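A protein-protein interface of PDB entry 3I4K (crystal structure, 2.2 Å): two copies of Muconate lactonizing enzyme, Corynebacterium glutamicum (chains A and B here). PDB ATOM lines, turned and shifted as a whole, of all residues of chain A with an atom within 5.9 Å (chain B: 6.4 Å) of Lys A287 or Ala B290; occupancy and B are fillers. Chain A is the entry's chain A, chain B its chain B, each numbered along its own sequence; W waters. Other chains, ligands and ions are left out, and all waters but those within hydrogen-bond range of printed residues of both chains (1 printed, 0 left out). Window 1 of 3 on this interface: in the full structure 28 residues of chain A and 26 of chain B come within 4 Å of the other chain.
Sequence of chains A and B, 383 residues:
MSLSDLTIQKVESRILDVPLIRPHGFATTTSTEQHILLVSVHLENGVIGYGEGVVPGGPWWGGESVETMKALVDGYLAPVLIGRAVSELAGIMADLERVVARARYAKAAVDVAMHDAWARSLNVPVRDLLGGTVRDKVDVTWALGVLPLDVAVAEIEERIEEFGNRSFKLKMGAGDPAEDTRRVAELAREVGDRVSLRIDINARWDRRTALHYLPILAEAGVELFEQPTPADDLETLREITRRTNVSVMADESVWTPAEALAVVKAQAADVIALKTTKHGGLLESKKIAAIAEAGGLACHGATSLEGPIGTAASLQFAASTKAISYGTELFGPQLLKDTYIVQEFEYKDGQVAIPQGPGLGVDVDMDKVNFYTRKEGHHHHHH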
ATOM      1  N   PRO A 257      -6.732 -11.112 -35.249  1.00  0.00           N
ATOM      2  CA  PRO A 257      -8.001 -11.360 -34.548  1.00  0.00           C
ATOM      3  C   PRO A 257      -9.056 -10.364 -35.027  1.00  0.00           C
ATOM      4  O   PRO A 257     -10.205 -10.729 -35.286  1.00  0.00           O
ATOM      5  CB  PRO A 257      -7.632 -11.139 -33.078  1.00  0.00           C
ATOM      6  CG  PRO A 257      -6.209 -11.666 -33.018  1.00  0.00           C
ATOM      7  CD  PRO A 257      -5.593 -11.094 -34.301  1.00  0.00           C
ATOM      8  N   ALA A 260     -10.322 -11.398 -38.207  1.00  0.00           N
ATOM      9  CA  ALA A 260     -11.187 -12.578 -38.114  1.00  0.00           C
ATOM     10  C   ALA A 260     -12.600 -12.115 -37.706  1.00  0.00           C
ATOM     11  O   ALA A 260     -13.614 -12.654 -38.164  1.00  0.00           O
ATOM     12  CB  ALA A 260     -10.642 -13.559 -37.086  1.00  0.00           C
ATOM     13  N   LEU A 282       1.801 -18.630 -31.929  1.00  0.00           N
ATOM     14  CA  LEU A 282       0.860 -19.598 -31.394  1.00  0.00           C
ATOM     15  C   LEU A 282      -0.166 -18.894 -30.488  1.00  0.00           C
ATOM     16  O   LEU A 282      -1.312 -19.322 -30.399  1.00  0.00           O
ATOM     17  CB  LEU A 282       1.618 -20.681 -30.619  1.00  0.00           C
ATOM     18  CG  LEU A 282       2.513 -21.570 -31.489  1.00  0.00           C
ATOM     19  CD1 LEU A 282       3.587 -22.226 -30.631  1.00  0.00           C
ATOM     20  CD2 LEU A 282       1.654 -22.628 -32.196  1.00  0.00           C
ATOM     21  N   LEU A 283       0.237 -17.816 -29.823  1.00  0.00           N
ATOM     22  CA  LEU A 283      -0.703 -17.102 -28.963  1.00  0.00           C
ATOM     23  C   LEU A 283      -1.779 -16.452 -29.841  1.00  0.00           C
ATOM     24  O   LEU A 283      -2.971 -16.631 -29.599  1.00  0.00           O
ATOM     25  CB  LEU A 283       0.005 -16.026 -28.116  1.00  0.00           C
ATOM     26  CG  LEU A 283       1.104 -16.479 -27.141  1.00  0.00           C
ATOM     27  CD1 LEU A 283       1.549 -15.295 -26.289  1.00  0.00           C
ATOM     28  CD2 LEU A 283       0.604 -17.602 -26.248  1.00  0.00           C
ATOM     29  N   GLU A 284      -1.357 -15.713 -30.862  1.00  0.00           N
ATOM     30  CA  GLU A 284      -2.299 -15.061 -31.766  1.00  0.00           C
ATOM     31  C   GLU A 284      -3.203 -16.075 -32.437  1.00  0.00           C
ATOM     32  O   GLU A 284      -4.403 -15.838 -32.575  1.00  0.00           O
ATOM     33  CB  GLU A 284      -1.561 -14.246 -32.828  1.00  0.00           C
ATOM     34  CG  GLU A 284      -0.917 -12.986 -32.274  1.00  0.00           C
ATOM     35  CD  GLU A 284      -1.925 -12.080 -31.578  1.00  0.00           C
ATOM     36  OE1 GLU A 284      -2.883 -11.640 -32.243  1.00  0.00           O
ATOM     37  OE2 GLU A 284      -1.765 -11.805 -30.373  1.00  0.00           O
ATOM     38  N   SER A 285      -2.629 -17.205 -32.842  1.00  0.00           N
ATOM     39  CA  SER A 285      -3.392 -18.264 -33.488  1.00  0.00           C
ATOM     40  C   SER A 285      -4.536 -18.759 -32.590  1.00  0.00           C
ATOM     41  O   SER A 285      -5.602 -19.130 -33.087  1.00  0.00           O
ATOM     42  CB  SER A 285      -2.478 -19.437 -33.848  1.00  0.00           C
ATOM     43  OG  SER A 285      -1.563 -19.090 -34.876  1.00  0.00           O
ATOM     44  N   LYS A 286      -4.312 -18.804 -31.278  1.00  0.00           N
ATOM     45  CA  LYS A 286      -5.377 -19.235 -30.360  1.00  0.00           C
ATOM     46  C   LYS A 286      -6.533 -18.238 -30.421  1.00  0.00           C
ATOM     47  O   LYS A 286      -7.706 -18.614 -30.317  1.00  0.00           O
ATOM     48  CB  LYS A 286      -4.876 -19.303 -28.911  1.00  0.00           C
ATOM     49  CG  LYS A 286      -4.157 -20.586 -28.532  1.00  0.00           C
ATOM     50  CD  LYS A 286      -5.057 -21.806 -28.694  1.00  0.00           C
ATOM     51  CE  LYS A 286      -4.392 -23.049 -28.140  1.00  0.00           C
ATOM     52  NZ  LYS A 286      -5.275 -24.233 -28.306  1.00  0.00           N
ATOM     53  N   LYS A 287      -6.189 -16.962 -30.583  1.00  0.00           N
ATOM     54  CA  LYS A 287      -7.200 -15.913 -30.651  1.00  0.00           C
ATOM     55  C   LYS A 287      -8.030 -16.045 -31.922  1.00  0.00           C
ATOM     56  O   LYS A 287      -9.255 -15.902 -31.886  1.00  0.00           O
ATOM     57  CB  LYS A 287      -6.538 -14.537 -30.581  1.00  0.00           C
ATOM     58  CG  LYS A 287      -5.687 -14.341 -29.323  1.00  0.00           C
ATOM     59  CD  LYS A 287      -5.128 -12.935 -29.263  1.00  0.00           C
ATOM     60  CE  LYS A 287      -4.153 -12.762 -28.110  1.00  0.00           C
ATOM     61  NZ  LYS A 287      -3.558 -11.402 -28.142  1.00  0.00           N
ATOM     62  N   ILE A 288      -7.371 -16.333 -33.043  1.00  0.00           N
ATOM     63  CA  ILE A 288      -8.093 -16.490 -34.305  1.00  0.00           C
ATOM     64  C   ILE A 288      -9.122 -17.601 -34.123  1.00  0.00           C
ATOM     65  O   ILE A 288     -10.286 -17.453 -34.486  1.00  0.00           O
ATOM     66  CB  ILE A 288      -7.155 -16.905 -35.480  1.00  0.00           C
ATOM     67  CG1 ILE A 288      -6.064 -15.853 -35.708  1.00  0.00           C
ATOM     68  CG2 ILE A 288      -7.986 -17.107 -36.749  1.00  0.00           C
ATOM     69  CD1 ILE A 288      -6.531 -14.521 -36.331  1.00  0.00           C
ATOM     70  N   ALA A 289      -8.683 -18.720 -33.555  1.00  0.00           N
ATOM     71  CA  ALA A 289      -9.565 -19.863 -33.349  1.00  0.00           C
ATOM     72  C   ALA A 289     -10.765 -19.542 -32.453  1.00  0.00           C
ATOM     73  O   ALA A 289     -11.893 -19.966 -32.734  1.00  0.00           O
ATOM     74  CB  ALA A 289      -8.774 -21.030 -32.764  1.00  0.00           C
ATOM     75  N   ALA A 290     -10.511 -18.805 -31.375  1.00  0.00           N
ATOM     76  CA  ALA A 290     -11.565 -18.430 -30.428  1.00  0.00           C
ATOM     77  C   ALA A 290     -12.664 -17.631 -31.122  1.00  0.00           C
ATOM     78  O   ALA A 290     -13.846 -17.906 -30.945  1.00  0.00           O
ATOM     79  CB  ALA A 290     -10.976 -17.599 -29.296  1.00  0.00           C
ATOM     80  N   ILE A 291     -12.253 -16.638 -31.908  1.00  0.00           N
ATOM     81  CA  ILE A 291     -13.199 -15.789 -32.617  1.00  0.00           C
ATOM     82  C   ILE A 291     -13.954 -16.591 -33.673  1.00  0.00           C
ATOM     83  O   ILE A 291     -15.178 -16.560 -33.720  1.00  0.00           O
ATOM     84  CB  ILE A 291     -12.465 -14.587 -33.240  1.00  0.00           C
ATOM     85  CG1 ILE A 291     -11.927 -13.699 -32.112  1.00  0.00           C
ATOM     86  CG2 ILE A 291     -13.394 -13.806 -34.164  1.00  0.00           C
ATOM     87  CD1 ILE A 291     -10.831 -12.745 -32.551  1.00  0.00           C
ATOM     88  N   ALA A 292     -13.230 -17.323 -34.510  1.00  0.00           N
ATOM     89  CA  ALA A 292     -13.875 -18.140 -35.538  1.00  0.00           C
ATOM     90  C   ALA A 292     -14.909 -19.088 -34.904  1.00  0.00           C
ATOM     91  O   ALA A 292     -16.077 -19.133 -35.315  1.00  0.00           O
ATOM     92  CB  ALA A 292     -12.814 -18.946 -36.298  1.00  0.00           C
ATOM     93  N   SER B 285     -12.094 -18.726 -20.631  1.00  0.00           N
ATOM     94  CA  SER B 285     -11.743 -17.350 -20.317  1.00  0.00           C
ATOM     95  C   SER B 285     -10.834 -16.754 -21.393  1.00  0.00           C
ATOM     96  O   SER B 285     -11.062 -15.637 -21.845  1.00  0.00           O
ATOM     97  CB  SER B 285     -11.070 -17.287 -18.950  1.00  0.00           C
ATOM     98  OG  SER B 285     -11.986 -17.671 -17.936  1.00  0.00           O
ATOM     99  N   LYS B 286      -9.813 -17.506 -21.808  1.00  0.00           N
ATOM    100  CA  LYS B 286      -8.898 -17.044 -22.848  1.00  0.00           C
ATOM    101  C   LYS B 286      -9.684 -16.608 -24.085  1.00  0.00           C
ATOM    102  O   LYS B 286      -9.345 -15.616 -24.735  1.00  0.00           O
ATOM    103  CB  LYS B 286      -7.928 -18.166 -23.255  1.00  0.00           C
ATOM    104  CG  LYS B 286      -6.747 -18.387 -22.323  1.00  0.00           C
ATOM    105  CD  LYS B 286      -5.830 -17.176 -22.294  1.00  0.00           C
ATOM    106  CE  LYS B 286      -4.613 -17.399 -21.398  1.00  0.00           C
ATOM    107  NZ  LYS B 286      -3.851 -16.124 -21.211  1.00  0.00           N
ATOM    108  N   LYS B 287     -10.726 -17.370 -24.406  1.00  0.00           N
ATOM    109  CA  LYS B 287     -11.560 -17.093 -25.568  1.00  0.00           C
ATOM    110  C   LYS B 287     -12.314 -15.780 -25.389  1.00  0.00           C
ATOM    111  O   LYS B 287     -12.367 -14.946 -26.302  1.00  0.00           O
ATOM    112  CB  LYS B 287     -12.533 -18.256 -25.785  1.00  0.00           C
ATOM    113  CG  LYS B 287     -11.839 -19.606 -25.985  1.00  0.00           C
ATOM    114  CD  LYS B 287     -12.877 -20.712 -26.210  1.00  0.00           C
ATOM    115  CE  LYS B 287     -12.240 -22.038 -26.554  1.00  0.00           C
ATOM    116  NZ  LYS B 287     -13.235 -23.149 -26.567  1.00  0.00           N
ATOM    117  N   ILE B 288     -12.887 -15.598 -24.204  1.00  0.00           N
ATOM    118  CA  ILE B 288     -13.609 -14.379 -23.884  1.00  0.00           C
ATOM    119  C   ILE B 288     -12.647 -13.219 -24.122  1.00  0.00           C
ATOM    120  O   ILE B 288     -12.962 -12.247 -24.817  1.00  0.00           O
ATOM    121  CB  ILE B 288     -14.053 -14.366 -22.388  1.00  0.00           C
ATOM    122  CG1 ILE B 288     -15.053 -15.505 -22.117  1.00  0.00           C
ATOM    123  CG2 ILE B 288     -14.617 -12.997 -22.019  1.00  0.00           C
ATOM    124  CD1 ILE B 288     -16.390 -15.414 -22.859  1.00  0.00           C
ATOM    125  N   ALA B 289     -11.457 -13.329 -23.550  1.00  0.00           N
ATOM    126  CA  ALA B 289     -10.454 -12.280 -23.681  1.00  0.00           C
ATOM    127  C   ALA B 289     -10.074 -11.976 -25.134  1.00  0.00           C
ATOM    128  O   ALA B 289      -9.908 -10.814 -25.509  1.00  0.00           O
ATOM    129  CB  ALA B 289      -9.210 -12.659 -22.883  1.00  0.00           C
ATOM    130  N   ALA B 290      -9.921 -13.019 -25.944  1.00  0.00           N
ATOM    131  CA  ALA B 290      -9.556 -12.842 -27.351  1.00  0.00           C
ATOM    132  C   ALA B 290     -10.627 -12.079 -28.145  1.00  0.00           C
ATOM    133  O   ALA B 290     -10.321 -11.178 -28.928  1.00  0.00           O
ATOM    134  CB  ALA B 290      -9.301 -14.211 -27.998  1.00  0.00           C
ATOM    135  N   ILE B 291     -11.886 -12.447 -27.952  1.00  0.00           N
ATOM    136  CA  ILE B 291     -12.977 -11.794 -28.669  1.00  0.00           C
ATOM    137  C   ILE B 291     -13.093 -10.327 -28.252  1.00  0.00           C
ATOM    138  O   ILE B 291     -13.148  -9.428 -29.098  1.00  0.00           O
ATOM    139  CB  ILE B 291     -14.292 -12.548 -28.400  1.00  0.00           C
ATOM    140  CG1 ILE B 291     -14.200 -13.927 -29.041  1.00  0.00           C
ATOM    141  CG2 ILE B 291     -15.482 -11.772 -28.927  1.00  0.00           C
ATOM    142  CD1 ILE B 291     -15.120 -14.949 -28.417  1.00  0.00           C
ATOM    143  N   ALA B 292     -13.109 -10.089 -26.946  1.00  0.00           N
ATOM    144  CA  ALA B 292     -13.209  -8.734 -26.408  1.00  0.00           C
ATOM    145  C   ALA B 292     -12.101  -7.851 -26.967  1.00  0.00           C
ATOM    146  O   ALA B 292     -12.357  -6.776 -27.521  1.00  0.00           O
ATOM    147  CB  ALA B 292     -13.129  -8.768 -24.867  1.00  0.00           C
ATOM    148  N   GLU B 293     -10.865  -8.315 -26.814  1.00  0.00           N
ATOM    149  CA  GLU B 293      -9.697  -7.586 -27.290  1.00  0.00           C
ATOM    150  C   GLU B 293      -9.781  -7.266 -28.776  1.00  0.00           C
ATOM    151  O   GLU B 293      -9.446  -6.158 -29.202  1.00  0.00           O
ATOM    152  CB  GLU B 293      -8.427  -8.405 -27.027  1.00  0.00           C
ATOM    153  CG  GLU B 293      -7.164  -7.785 -27.592  1.00  0.00           C
ATOM    154  CD  GLU B 293      -5.921  -8.602 -27.273  1.00  0.00           C
ATOM    155  OE1 GLU B 293      -5.863  -9.792 -27.648  1.00  0.00           O
ATOM    156  OE2 GLU B 293      -4.999  -8.046 -26.639  1.00  0.00           O
ATOM    157  N   ALA B 294     -10.216  -8.232 -29.572  1.00  0.00           N
ATOM    158  CA  ALA B 294     -10.312  -8.000 -31.015  1.00  0.00           C
ATOM    159  C   ALA B 294     -11.355  -6.915 -31.328  1.00  0.00           C
ATOM    160  O   ALA B 294     -11.233  -6.193 -32.313  1.00  0.00           O
ATOM    161  CB  ALA B 294     -10.657  -9.310 -31.738  1.00  0.00           C
ATOM    162  N   GLY B 295     -12.361  -6.785 -30.469  1.00  0.00           N
ATOM    163  CA  GLY B 295     -13.401  -5.789 -30.683  1.00  0.00           C
ATOM    164  C   GLY B 295     -13.138  -4.494 -29.943  1.00  0.00           C
ATOM    165  O   GLY B 295     -13.993  -3.609 -29.906  1.00  0.00           O
ATOM    166  N   CYS B 299     -11.293  -5.767 -20.682  1.00  0.00           N
ATOM    167  CA  CYS B 299     -11.678  -6.872 -19.806  1.00  0.00           C
ATOM    168  C   CYS B 299     -11.270  -6.568 -18.379  1.00  0.00           C
ATOM    169  O   CYS B 299     -10.138  -6.155 -18.112  1.00  0.00           O
ATOM    170  CB  CYS B 299     -11.026  -8.191 -20.228  1.00  0.00           C
ATOM    171  SG  CYS B 299     -11.743  -8.978 -21.686  1.00  0.00           S
ATOM    172  N   THR B 321      -2.730 -12.699 -19.045  1.00  0.00           N
ATOM    173  CA  THR B 321      -3.590 -12.116 -20.070  1.00  0.00           C
ATOM    174  C   THR B 321      -3.545 -10.606 -20.170  1.00  0.00           C
ATOM    175  O   THR B 321      -4.142  -9.904 -19.358  1.00  0.00           O
ATOM    176  CB  THR B 321      -5.042 -12.563 -19.835  1.00  0.00           C
ATOM    177  OG1 THR B 321      -5.047 -13.964 -19.548  1.00  0.00           O
ATOM    178  CG2 THR B 321      -5.906 -12.308 -21.073  1.00  0.00           C
ATOM    179  N   ALA B 323      -5.041  -8.869 -22.158  1.00  0.00           N
ATOM    180  CA  ALA B 323      -6.400  -8.396 -22.418  1.00  0.00           C
ATOM    181  C   ALA B 323      -7.122  -7.913 -21.149  1.00  0.00           C
ATOM    182  O   ALA B 323      -8.112  -7.191 -21.238  1.00  0.00           O
ATOM    183  CB  ALA B 323      -7.214  -9.482 -23.125  1.00  0.00           C
HETATM  184  O   HOH W   1      -2.977  -9.589 -25.795  1.00  0.00           O
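The side-chain amino group of Lys A287 is in salt-bridge range of the side-chain carboxylate of Glu B293 (2.9 Å).
The side-chain carboxylate (OE2) of Glu A284 lies within salt-bridge range of the side-chain amino group (NZ) of Lys A287, at 2.9 Å.
Among the printed residues, merely in contact across the chains: Ile A291 with Ala B294 (3.5 Å), Pro A257 with Ala B294 (3.8 Å), Lys A287 with Ala B290 (3.8 Å), Ala A290 with Lys B287 (3.8 Å), Ile A291 with Ile B291 (3.8 Å), Ile A291 with Ala B290 (3.98 Å) and Ala A290 with Ala B290 (3.996 Å).
Of the printed residues of chain B, Pro A257 touches Ala B294. Leu A282 touches none of the printed residues of chain B. Of chain B, only Ala B290 (3.8 Å) and Glu B293 (2.9 Å) come within 4 Å of Lys A287. Of the printed residues of chain B, Ala A290 touches Lys B287 and Ala B290. Of the printed residues of chain A, Lys B287 touches Ala A290. Of the printed residues of chain A, Ala B290 touches Lys A287, Ala A290 and Ile A291. Printed residues of chain A within 4 Å of Ile B291: Ile A291. Printed residues of chain A within 4 Å of Ala B294: Pro A257 and Ile A291. The nearest residue of chain B that does not touch Lys A287 is Ile B291 (5.9 Å). The nearest printed residue of chain A that does not touch Ala B290 is Pro A257 (4.9 Å).
Of the 13 printed residues of chain A, 4 touch a printed residue of chain B. Hydrophobic or aromatic side chains of chain A that line the printed part of chain B: Pro A257, Ala A290 and Ile A291. Among the printed residues, 8 pairs touch across the chains. Among the printed residues, Asp or Glu carboxylates within 4 Å of a Lys or Arg side-chain nitrogen of the other chain: Lys A287 with Glu B293.
Lys A287 touches Ala B290, and with the chains exchanged Ala A290 touches Lys B287. Ala A290 touches its own counterpart, Ala B290. Ile A291 touches Ala B290, but with the chains exchanged Ala A290 does not touch Ile B291 (4.1 Å). Ile B291 touches its own counterpart, Ile A291. Of the 8 pairs that touch across the chains among the printed residues, 4 have their exchanged pair printed and touching as well.
Water W1 bridges OE2 of Glu B293 (2.7 Å) and NZ of Lys A287 (3.0 Å).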
